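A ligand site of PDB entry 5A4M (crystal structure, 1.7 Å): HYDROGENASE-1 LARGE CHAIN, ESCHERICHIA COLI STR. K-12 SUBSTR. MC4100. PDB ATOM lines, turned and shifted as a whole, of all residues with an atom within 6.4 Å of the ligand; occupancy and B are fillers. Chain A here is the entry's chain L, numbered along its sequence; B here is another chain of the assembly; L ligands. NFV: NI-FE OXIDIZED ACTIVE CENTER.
The backbone nitrogen of Pro 508 sits close to a nitrogen (N3) of the ligand (3.4 Å).
Residues that only touch the ligand: Val 82 (3.5 Å), Ala 507 (3.3 Å), Leu 512 (3.5 Å), Val 530 (3.4 Å) and Pro 531 (3.5 Å).
Hydrophobic or aromatic side chains within 4 Å of the ligand: Val 82, His 83, Ala 507, Pro 508, Leu 512, Val 530 and Pro 531.
Of the 29 residues printed, 13 come within 4 Å of the ligand.
The backbone NH of Cys 576 lies within hydrogen-bond range of the side-chain hydroxyl of Thr 532 (3.2 Å).
The side-chain sulfur (SG) of Cys 579 lies close to a ring nitrogen (NE2) of His 83 (3.4 Å).
The side-chain sulfur (SG) of Cys 76 lies close to the backbone NH (N) of Val 78 (3.5 Å).
The side-chain carboxylate of Asp 118 is in salt-bridge range of the guanidinium group of Arg 509, at 2.8 Å.
The side-chain carboxylate (OD1) of Asp 574 is in salt-bridge range of the guanidinium group (NH2) of Arg 509.
The side-chain hydroxyl of Thr 533 sits close to the backbone carbonyl oxygen of Val 530.
A nickel atom (NI) of the ligand is bound by the side-chain sulfur of Cys 576.
SG of Cys 579 is bound to FE of the ligand, 2.3 Å away.
The side-chain sulfur (SG) of Cys 76 binds a nickel atom (NI) of the ligand, 2.3 Å away.
An iron atom (FE) of the ligand is bound by the side-chain sulfur of Cys 79.
N of Thr 532 sits at hydrogen-bond distance from N2 of the ligand, 3.0 Å away.
The side-chain hydroxyl (OG1) of Thr 532 lies within hydrogen-bond range of a nitrogen (N2) of the ligand (2.8 Å).
N3 of the ligand lies within hydrogen-bond range of N of Arg 509, 3.0 Å away.
N3 of the ligand lies within hydrogen-bond range of NH1 of Arg 509 (3.2 Å).
A ring nitrogen (NE2) of His 83 lies within hydrogen-bond range of an oxygen (O1) of the ligand (3.4 Å).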
ATOM      1  N   GLU A  28      15.757  20.956  19.543  1.00  0.00           N
ATOM      2  CA  GLU A  28      15.423  20.763  18.122  1.00  0.00           C
ATOM      3  C   GLU A  28      15.931  19.372  17.688  1.00  0.00           C
ATOM      4  O   GLU A  28      17.078  19.001  18.009  1.00  0.00           O
ATOM      5  CB  GLU A  28      16.114  21.812  17.237  1.00  0.00           C
ATOM      6  CG  GLU A  28      15.614  21.808  15.809  1.00  0.00           C
ATOM      7  CD  GLU A  28      16.008  20.591  15.002  1.00  0.00           C
ATOM      8  OE1 GLU A  28      17.123  20.059  15.289  1.00  0.00           O
ATOM      9  OE2 GLU A  28      15.172  20.083  14.202  1.00  0.00           O
ATOM     10  N   ILE A  75      18.718  23.203   6.768  1.00  0.00           N
ATOM     11  CA  ILE A  75      19.407  22.375   7.814  1.00  0.00           C
ATOM     12  C   ILE A  75      18.652  22.598   9.093  1.00  0.00           C
ATOM     13  O   ILE A  75      18.502  21.685   9.907  1.00  0.00           O
ATOM     14  CB  ILE A  75      20.886  22.768   7.964  1.00  0.00           C
ATOM     15  CG1 ILE A  75      21.643  22.200   6.742  1.00  0.00           C
ATOM     16  CG2 ILE A  75      21.408  22.229   9.267  1.00  0.00           C
ATOM     17  CD1 ILE A  75      23.076  22.645   6.627  1.00  0.00           C
ATOM     18  N   CYS A  76      18.169  23.845   9.327  1.00  0.00           N
ATOM     19  CA  CYS A  76      17.516  24.092  10.575  1.00  0.00           C
ATOM     20  C   CYS A  76      16.573  25.311  10.627  1.00  0.00           C
ATOM     21  O   CYS A  76      16.890  26.322  10.088  1.00  0.00           O
ATOM     22  CB  CYS A  76      18.473  24.343  11.644  1.00  0.00           C
ATOM     23  SG  CYS A  76      17.634  24.009  13.258  1.00  0.00           S
ATOM     24  N   GLY A  77      15.441  25.128  11.247  1.00  0.00           N
ATOM     25  CA  GLY A  77      14.392  26.132  11.264  1.00  0.00           C
ATOM     26  C   GLY A  77      14.403  26.930  12.568  1.00  0.00           C
ATOM     27  O   GLY A  77      13.778  27.972  12.660  1.00  0.00           O
ATOM     28  N   VAL A  78      15.194  26.487  13.534  1.00  0.00           N
ATOM     29  CA  VAL A  78      15.375  27.149  14.817  1.00  0.00           C
ATOM     30  C   VAL A  78      16.437  28.264  14.677  1.00  0.00           C
ATOM     31  O   VAL A  78      16.148  29.443  14.836  1.00  0.00           O
ATOM     32  CB  VAL A  78      15.714  26.127  15.919  1.00  0.00           C
ATOM     33  CG1 VAL A  78      15.875  26.824  17.221  1.00  0.00           C
ATOM     34  CG2 VAL A  78      14.576  25.117  16.017  1.00  0.00           C
ATOM     35  N   CYS A  79      17.623  27.892  14.255  1.00  0.00           N
ATOM     36  CA  CYS A  79      18.669  28.858  13.892  1.00  0.00           C
ATOM     37  C   CYS A  79      18.472  29.299  12.444  1.00  0.00           C
ATOM     38  O   CYS A  79      19.428  29.464  11.692  1.00  0.00           O
ATOM     39  CB  CYS A  79      20.091  28.316  14.157  1.00  0.00           C
ATOM     40  SG  CYS A  79      20.513  26.759  13.330  1.00  0.00           S
ATOM     41  N   THR A  80      17.224  29.634  12.073  1.00  0.00           N
ATOM     42  CA  THR A  80      16.912  29.905  10.678  1.00  0.00           C
ATOM     43  C   THR A  80      17.617  31.189  10.199  1.00  0.00           C
ATOM     44  O   THR A  80      17.586  32.250  10.841  1.00  0.00           O
ATOM     45  CB  THR A  80      15.364  30.006  10.443  1.00  0.00           C
ATOM     46  OG1 THR A  80      15.131  30.223   9.052  1.00  0.00           O
ATOM     47  CG2 THR A  80      14.762  31.194  11.197  1.00  0.00           C
ATOM     48  N   VAL A  82      21.009  31.346   9.650  1.00  0.00           N
ATOM     49  CA  VAL A  82      22.450  31.326   9.852  1.00  0.00           C
ATOM     50  C   VAL A  82      23.213  30.491   8.818  1.00  0.00           C
ATOM     51  O   VAL A  82      24.299  30.864   8.405  1.00  0.00           O
ATOM     52  CB  VAL A  82      22.806  30.927  11.297  1.00  0.00           C
ATOM     53  CG1 VAL A  82      22.711  29.444  11.523  1.00  0.00           C
ATOM     54  CG2 VAL A  82      24.174  31.462  11.561  1.00  0.00           C
ATOM     55  N   HIS A  83      22.605  29.395   8.343  1.00  0.00           N
ATOM     56  CA  HIS A  83      23.191  28.579   7.317  1.00  0.00           C
ATOM     57  C   HIS A  83      23.164  29.295   5.977  1.00  0.00           C
ATOM     58  O   HIS A  83      24.090  29.152   5.169  1.00  0.00           O
ATOM     59  CB  HIS A  83      22.515  27.213   7.218  1.00  0.00           C
ATOM     60  CG  HIS A  83      22.799  26.324   8.384  1.00  0.00           C
ATOM     61  ND1 HIS A  83      24.063  25.765   8.587  1.00  0.00           N
ATOM     62  CD2 HIS A  83      22.045  25.962   9.444  1.00  0.00           C
ATOM     63  CE1 HIS A  83      24.040  25.047   9.690  1.00  0.00           C
ATOM     64  NE2 HIS A  83      22.846  25.166  10.240  1.00  0.00           N
ATOM     65  N   LEU A 114      18.267  37.056  14.726  1.00  0.00           N
ATOM     66  CA  LEU A 114      18.234  35.631  15.056  1.00  0.00           C
ATOM     67  C   LEU A 114      18.773  35.341  16.486  1.00  0.00           C
ATOM     68  O   LEU A 114      18.194  34.573  17.232  1.00  0.00           O
ATOM     69  CB  LEU A 114      19.018  34.836  14.023  1.00  0.00           C
ATOM     70  CG  LEU A 114      19.109  33.330  14.403  1.00  0.00           C
ATOM     71  CD1 LEU A 114      17.682  32.701  14.275  1.00  0.00           C
ATOM     72  CD2 LEU A 114      20.070  32.591  13.516  1.00  0.00           C
ATOM     73  N   ASP A 118      16.290  33.531  18.952  1.00  0.00           N
ATOM     74  CA  ASP A 118      16.655  32.189  19.335  1.00  0.00           C
ATOM     75  C   ASP A 118      17.029  32.051  20.803  1.00  0.00           C
ATOM     76  O   ASP A 118      16.548  31.118  21.514  1.00  0.00           O
ATOM     77  CB  ASP A 118      17.795  31.793  18.401  1.00  0.00           C
ATOM     78  CG  ASP A 118      18.017  30.317  18.315  1.00  0.00           C
ATOM     79  OD1 ASP A 118      17.718  29.569  19.306  1.00  0.00           O
ATOM     80  OD2 ASP A 118      18.546  29.880  17.216  1.00  0.00           O
ATOM     81  N   ALA A 507      26.775  31.174  15.068  1.00  0.00           N
ATOM     82  CA  ALA A 507      25.372  30.963  15.177  1.00  0.00           C
ATOM     83  C   ALA A 507      25.002  31.010  16.648  1.00  0.00           C
ATOM     84  O   ALA A 507      25.901  31.006  17.516  1.00  0.00           O
ATOM     85  CB  ALA A 507      25.027  29.589  14.592  1.00  0.00           C
ATOM     86  N   PRO A 508      23.716  31.072  16.986  1.00  0.00           N
ATOM     87  CA  PRO A 508      23.337  31.100  18.420  1.00  0.00           C
ATOM     88  C   PRO A 508      23.970  30.032  19.314  1.00  0.00           C
ATOM     89  O   PRO A 508      24.376  30.325  20.432  1.00  0.00           O
ATOM     90  CB  PRO A 508      21.819  30.978  18.394  1.00  0.00           C
ATOM     91  CG  PRO A 508      21.461  31.649  17.066  1.00  0.00           C
ATOM     92  CD  PRO A 508      22.554  31.342  16.108  1.00  0.00           C
ATOM     93  N   ARG A 509      24.225  28.851  18.752  1.00  0.00           N
ATOM     94  CA  ARG A 509      24.781  27.725  19.482  1.00  0.00           C
ATOM     95  C   ARG A 509      26.292  27.570  19.393  1.00  0.00           C
ATOM     96  O   ARG A 509      26.847  26.728  20.095  1.00  0.00           O
ATOM     97  CB  ARG A 509      24.079  26.450  19.160  1.00  0.00           C
ATOM     98  CG  ARG A 509      22.557  26.525  19.507  1.00  0.00           C
ATOM     99  CD  ARG A 509      21.769  25.518  18.704  1.00  0.00           C
ATOM    100  NE  ARG A 509      20.382  25.693  19.117  1.00  0.00           N
ATOM    101  CZ  ARG A 509      19.599  26.679  18.711  1.00  0.00           C
ATOM    102  NH1 ARG A 509      19.954  27.517  17.749  1.00  0.00           N
ATOM    103  NH2 ARG A 509      18.376  26.801  19.256  1.00  0.00           N
ATOM    104  N   GLY A 510      26.942  28.402  18.565  1.00  0.00           N
ATOM    105  CA  GLY A 510      28.387  28.371  18.430  1.00  0.00           C
ATOM    106  C   GLY A 510      28.955  28.519  17.042  1.00  0.00           C
ATOM    107  O   GLY A 510      28.310  28.983  16.109  1.00  0.00           O
ATOM    108  N   ALA A 511      30.189  28.060  16.888  1.00  0.00           N
ATOM    109  CA  ALA A 511      30.983  28.240  15.672  1.00  0.00           C
ATOM    110  C   ALA A 511      30.484  27.381  14.512  1.00  0.00           C
ATOM    111  O   ALA A 511      30.415  26.177  14.603  1.00  0.00           O
ATOM    112  CB  ALA A 511      32.431  27.853  15.983  1.00  0.00           C
ATOM    113  N   LEU A 512      30.153  28.050  13.415  1.00  0.00           N
ATOM    114  CA  LEU A 512      29.589  27.454  12.211  1.00  0.00           C
ATOM    115  C   LEU A 512      30.495  27.703  11.037  1.00  0.00           C
ATOM    116  O   LEU A 512      30.938  28.822  10.779  1.00  0.00           O
ATOM    117  CB  LEU A 512      28.240  28.149  11.881  1.00  0.00           C
ATOM    118  CG  LEU A 512      27.576  27.640  10.591  1.00  0.00           C
ATOM    119  CD1 LEU A 512      27.272  26.150  10.588  1.00  0.00           C
ATOM    120  CD2 LEU A 512      26.311  28.421  10.379  1.00  0.00           C
ATOM    121  N   VAL A 530      28.945  22.202  12.208  1.00  0.00           N
ATOM    122  CA  VAL A 530      27.950  23.075  12.817  1.00  0.00           C
ATOM    123  C   VAL A 530      28.122  23.038  14.328  1.00  0.00           C
ATOM    124  O   VAL A 530      28.766  22.136  14.869  1.00  0.00           O
ATOM    125  CB  VAL A 530      26.570  22.542  12.330  1.00  0.00           C
ATOM    126  CG1 VAL A 530      25.442  23.403  12.697  1.00  0.00           C
ATOM    127  CG2 VAL A 530      26.542  22.413  10.806  1.00  0.00           C
ATOM    128  N   PRO A 531      27.677  24.068  15.045  1.00  0.00           N
ATOM    129  CA  PRO A 531      28.034  24.103  16.453  1.00  0.00           C
ATOM    130  C   PRO A 531      27.632  22.894  17.268  1.00  0.00           C
ATOM    131  O   PRO A 531      28.431  22.419  18.084  1.00  0.00           O
ATOM    132  CB  PRO A 531      27.320  25.344  16.984  1.00  0.00           C
ATOM    133  CG  PRO A 531      26.795  26.043  15.824  1.00  0.00           C
ATOM    134  CD  PRO A 531      27.103  25.331  14.617  1.00  0.00           C
ATOM    135  N   THR A 532      26.421  22.363  17.079  1.00  0.00           N
ATOM    136  CA  THR A 532      26.069  21.178  17.862  1.00  0.00           C
ATOM    137  C   THR A 532      26.846  19.972  17.377  1.00  0.00           C
ATOM    138  O   THR A 532      26.966  18.984  18.093  1.00  0.00           O
ATOM    139  CB  THR A 532      24.539  21.009  17.854  1.00  0.00           C
ATOM    140  OG1 THR A 532      23.930  22.203  18.414  1.00  0.00           O
ATOM    141  CG2 THR A 532      24.118  19.786  18.655  1.00  0.00           C
ATOM    142  N   THR A 533      27.368  19.975  16.180  1.00  0.00           N
ATOM    143  CA  THR A 533      28.276  18.853  15.793  1.00  0.00           C
ATOM    144  C   THR A 533      29.453  18.831  16.790  1.00  0.00           C
ATOM    145  O   THR A 533      29.868  17.773  17.238  1.00  0.00           O
ATOM    146  CB  THR A 533      28.809  19.001  14.370  1.00  0.00           C
ATOM    147  OG1 THR A 533      27.790  19.400  13.429  1.00  0.00           O
ATOM    148  CG2 THR A 533      29.467  17.731  13.925  1.00  0.00           C
ATOM    149  N   ASP A 574      21.766  24.324  24.568  1.00  0.00           N
ATOM    150  CA  ASP A 574      20.744  24.546  23.467  1.00  0.00           C
ATOM    151  C   ASP A 574      20.988  23.589  22.252  1.00  0.00           C
ATOM    152  O   ASP A 574      21.372  24.063  21.160  1.00  0.00           O
ATOM    153  CB  ASP A 574      20.849  26.024  23.076  1.00  0.00           C
ATOM    154  CG  ASP A 574      19.826  26.495  22.126  1.00  0.00           C
ATOM    155  OD1 ASP A 574      18.844  25.770  21.790  1.00  0.00           O
ATOM    156  OD2 ASP A 574      20.061  27.670  21.723  1.00  0.00           O
ATOM    157  N   PRO A 575      20.841  22.265  22.435  1.00  0.00           N
ATOM    158  CA  PRO A 575      21.130  21.268  21.372  1.00  0.00           C
ATOM    159  C   PRO A 575      20.200  21.495  20.152  1.00  0.00           C
ATOM    160  O   PRO A 575      19.001  21.632  20.270  1.00  0.00           O
ATOM    161  CB  PRO A 575      20.878  19.932  22.024  1.00  0.00           C
ATOM    162  CG  PRO A 575      21.023  20.222  23.476  1.00  0.00           C
ATOM    163  CD  PRO A 575      20.458  21.583  23.668  1.00  0.00           C
ATOM    164  N   CYS A 576      20.844  21.502  18.994  1.00  0.00           N
ATOM    165  CA  CYS A 576      20.126  21.587  17.705  1.00  0.00           C
ATOM    166  C   CYS A 576      20.596  20.364  16.927  1.00  0.00           C
ATOM    167  O   CYS A 576      21.652  20.354  16.305  1.00  0.00           O
ATOM    168  CB  CYS A 576      20.428  22.884  16.946  1.00  0.00           C
ATOM    169  SG  CYS A 576      19.128  22.789  15.598  1.00  0.00           S
ATOM    170  N   LEU A 577      19.814  19.293  17.002  1.00  0.00           N
ATOM    171  CA  LEU A 577      20.270  18.035  16.405  1.00  0.00           C
ATOM    172  C   LEU A 577      20.190  17.980  14.891  1.00  0.00           C
ATOM    173  O   LEU A 577      20.996  17.290  14.270  1.00  0.00           O
ATOM    174  CB  LEU A 577      19.557  16.845  17.017  1.00  0.00           C
ATOM    175  CG  LEU A 577      20.180  16.431  18.377  1.00  0.00           C
ATOM    176  CD1 LEU A 577      21.470  15.677  18.192  1.00  0.00           C
ATOM    177  CD2 LEU A 577      20.382  17.566  19.377  1.00  0.00           C
ATOM    178  N   ALA A 578      19.201  18.627  14.311  1.00  0.00           N
ATOM    179  CA  ALA A 578      19.139  18.771  12.838  1.00  0.00           C
ATOM    180  C   ALA A 578      20.348  19.495  12.326  1.00  0.00           C
ATOM    181  O   ALA A 578      20.964  19.086  11.342  1.00  0.00           O
ATOM    182  CB  ALA A 578      17.908  19.490  12.444  1.00  0.00           C
ATOM    183  N   CYS A 579      20.745  20.573  13.003  1.00  0.00           N
ATOM    184  CA  CYS A 579      21.998  21.219  12.678  1.00  0.00           C
ATOM    185  C   CYS A 579      23.146  20.227  12.775  1.00  0.00           C
ATOM    186  O   CYS A 579      24.068  20.267  11.934  1.00  0.00           O
ATOM    187  CB  CYS A 579      22.303  22.392  13.645  1.00  0.00           C
ATOM    188  SG  CYS A 579      21.544  23.941  13.119  1.00  0.00           S
ATOM    189  N   SER A 580      23.197  19.489  13.868  1.00  0.00           N
ATOM    190  CA  SER A 580      24.410  18.719  14.150  1.00  0.00           C
ATOM    191  C   SER A 580      24.733  17.697  13.094  1.00  0.00           C
ATOM    192  O   SER A 580      25.904  17.353  12.926  1.00  0.00           O
ATOM    193  CB  SER A 580      24.299  18.001  15.535  1.00  0.00           C
ATOM    194  OG  SER A 580      23.404  16.909  15.509  1.00  0.00           O
ATOM    195  N   CYS B  17      13.469  19.997  10.005  1.00  0.00           N
ATOM    196  CA  CYS B  17      14.314  21.043  10.516  1.00  0.00           C
ATOM    197  C   CYS B  17      13.605  21.869  11.584  1.00  0.00           C
ATOM    198  O   CYS B  17      14.215  22.718  12.142  1.00  0.00           O
ATOM    199  CB  CYS B  17      14.757  21.895   9.353  1.00  0.00           C
ATOM    200  SG  CYS B  17      13.670  23.265   8.867  1.00  0.00           S
HETATM  201 FE   NFV L   1      22.201  25.649  14.445  1.00  0.00          FE
HETATM  202 NI   NFV L   1      19.530  24.616  14.393  1.00  0.00          NI
HETATM  203  C1  NFV L   1      23.678  26.295  13.589  1.00  0.00           C
HETATM  204  O1  NFV L   1      24.472  26.675  12.817  1.00  0.00           O
HETATM  205  C2  NFV L   1      23.301  24.565  15.515  1.00  0.00           C
HETATM  206  N2  NFV L   1      23.965  23.903  16.174  1.00  0.00           N
HETATM  207  C3  NFV L   1      22.560  27.012  15.561  1.00  0.00           C
HETATM  208  N3  NFV L   1      22.723  27.918  16.271  1.00  0.00           N
HETATM  209  O4  NFV L   1      20.802  25.509  15.690  1.00  0.00           O
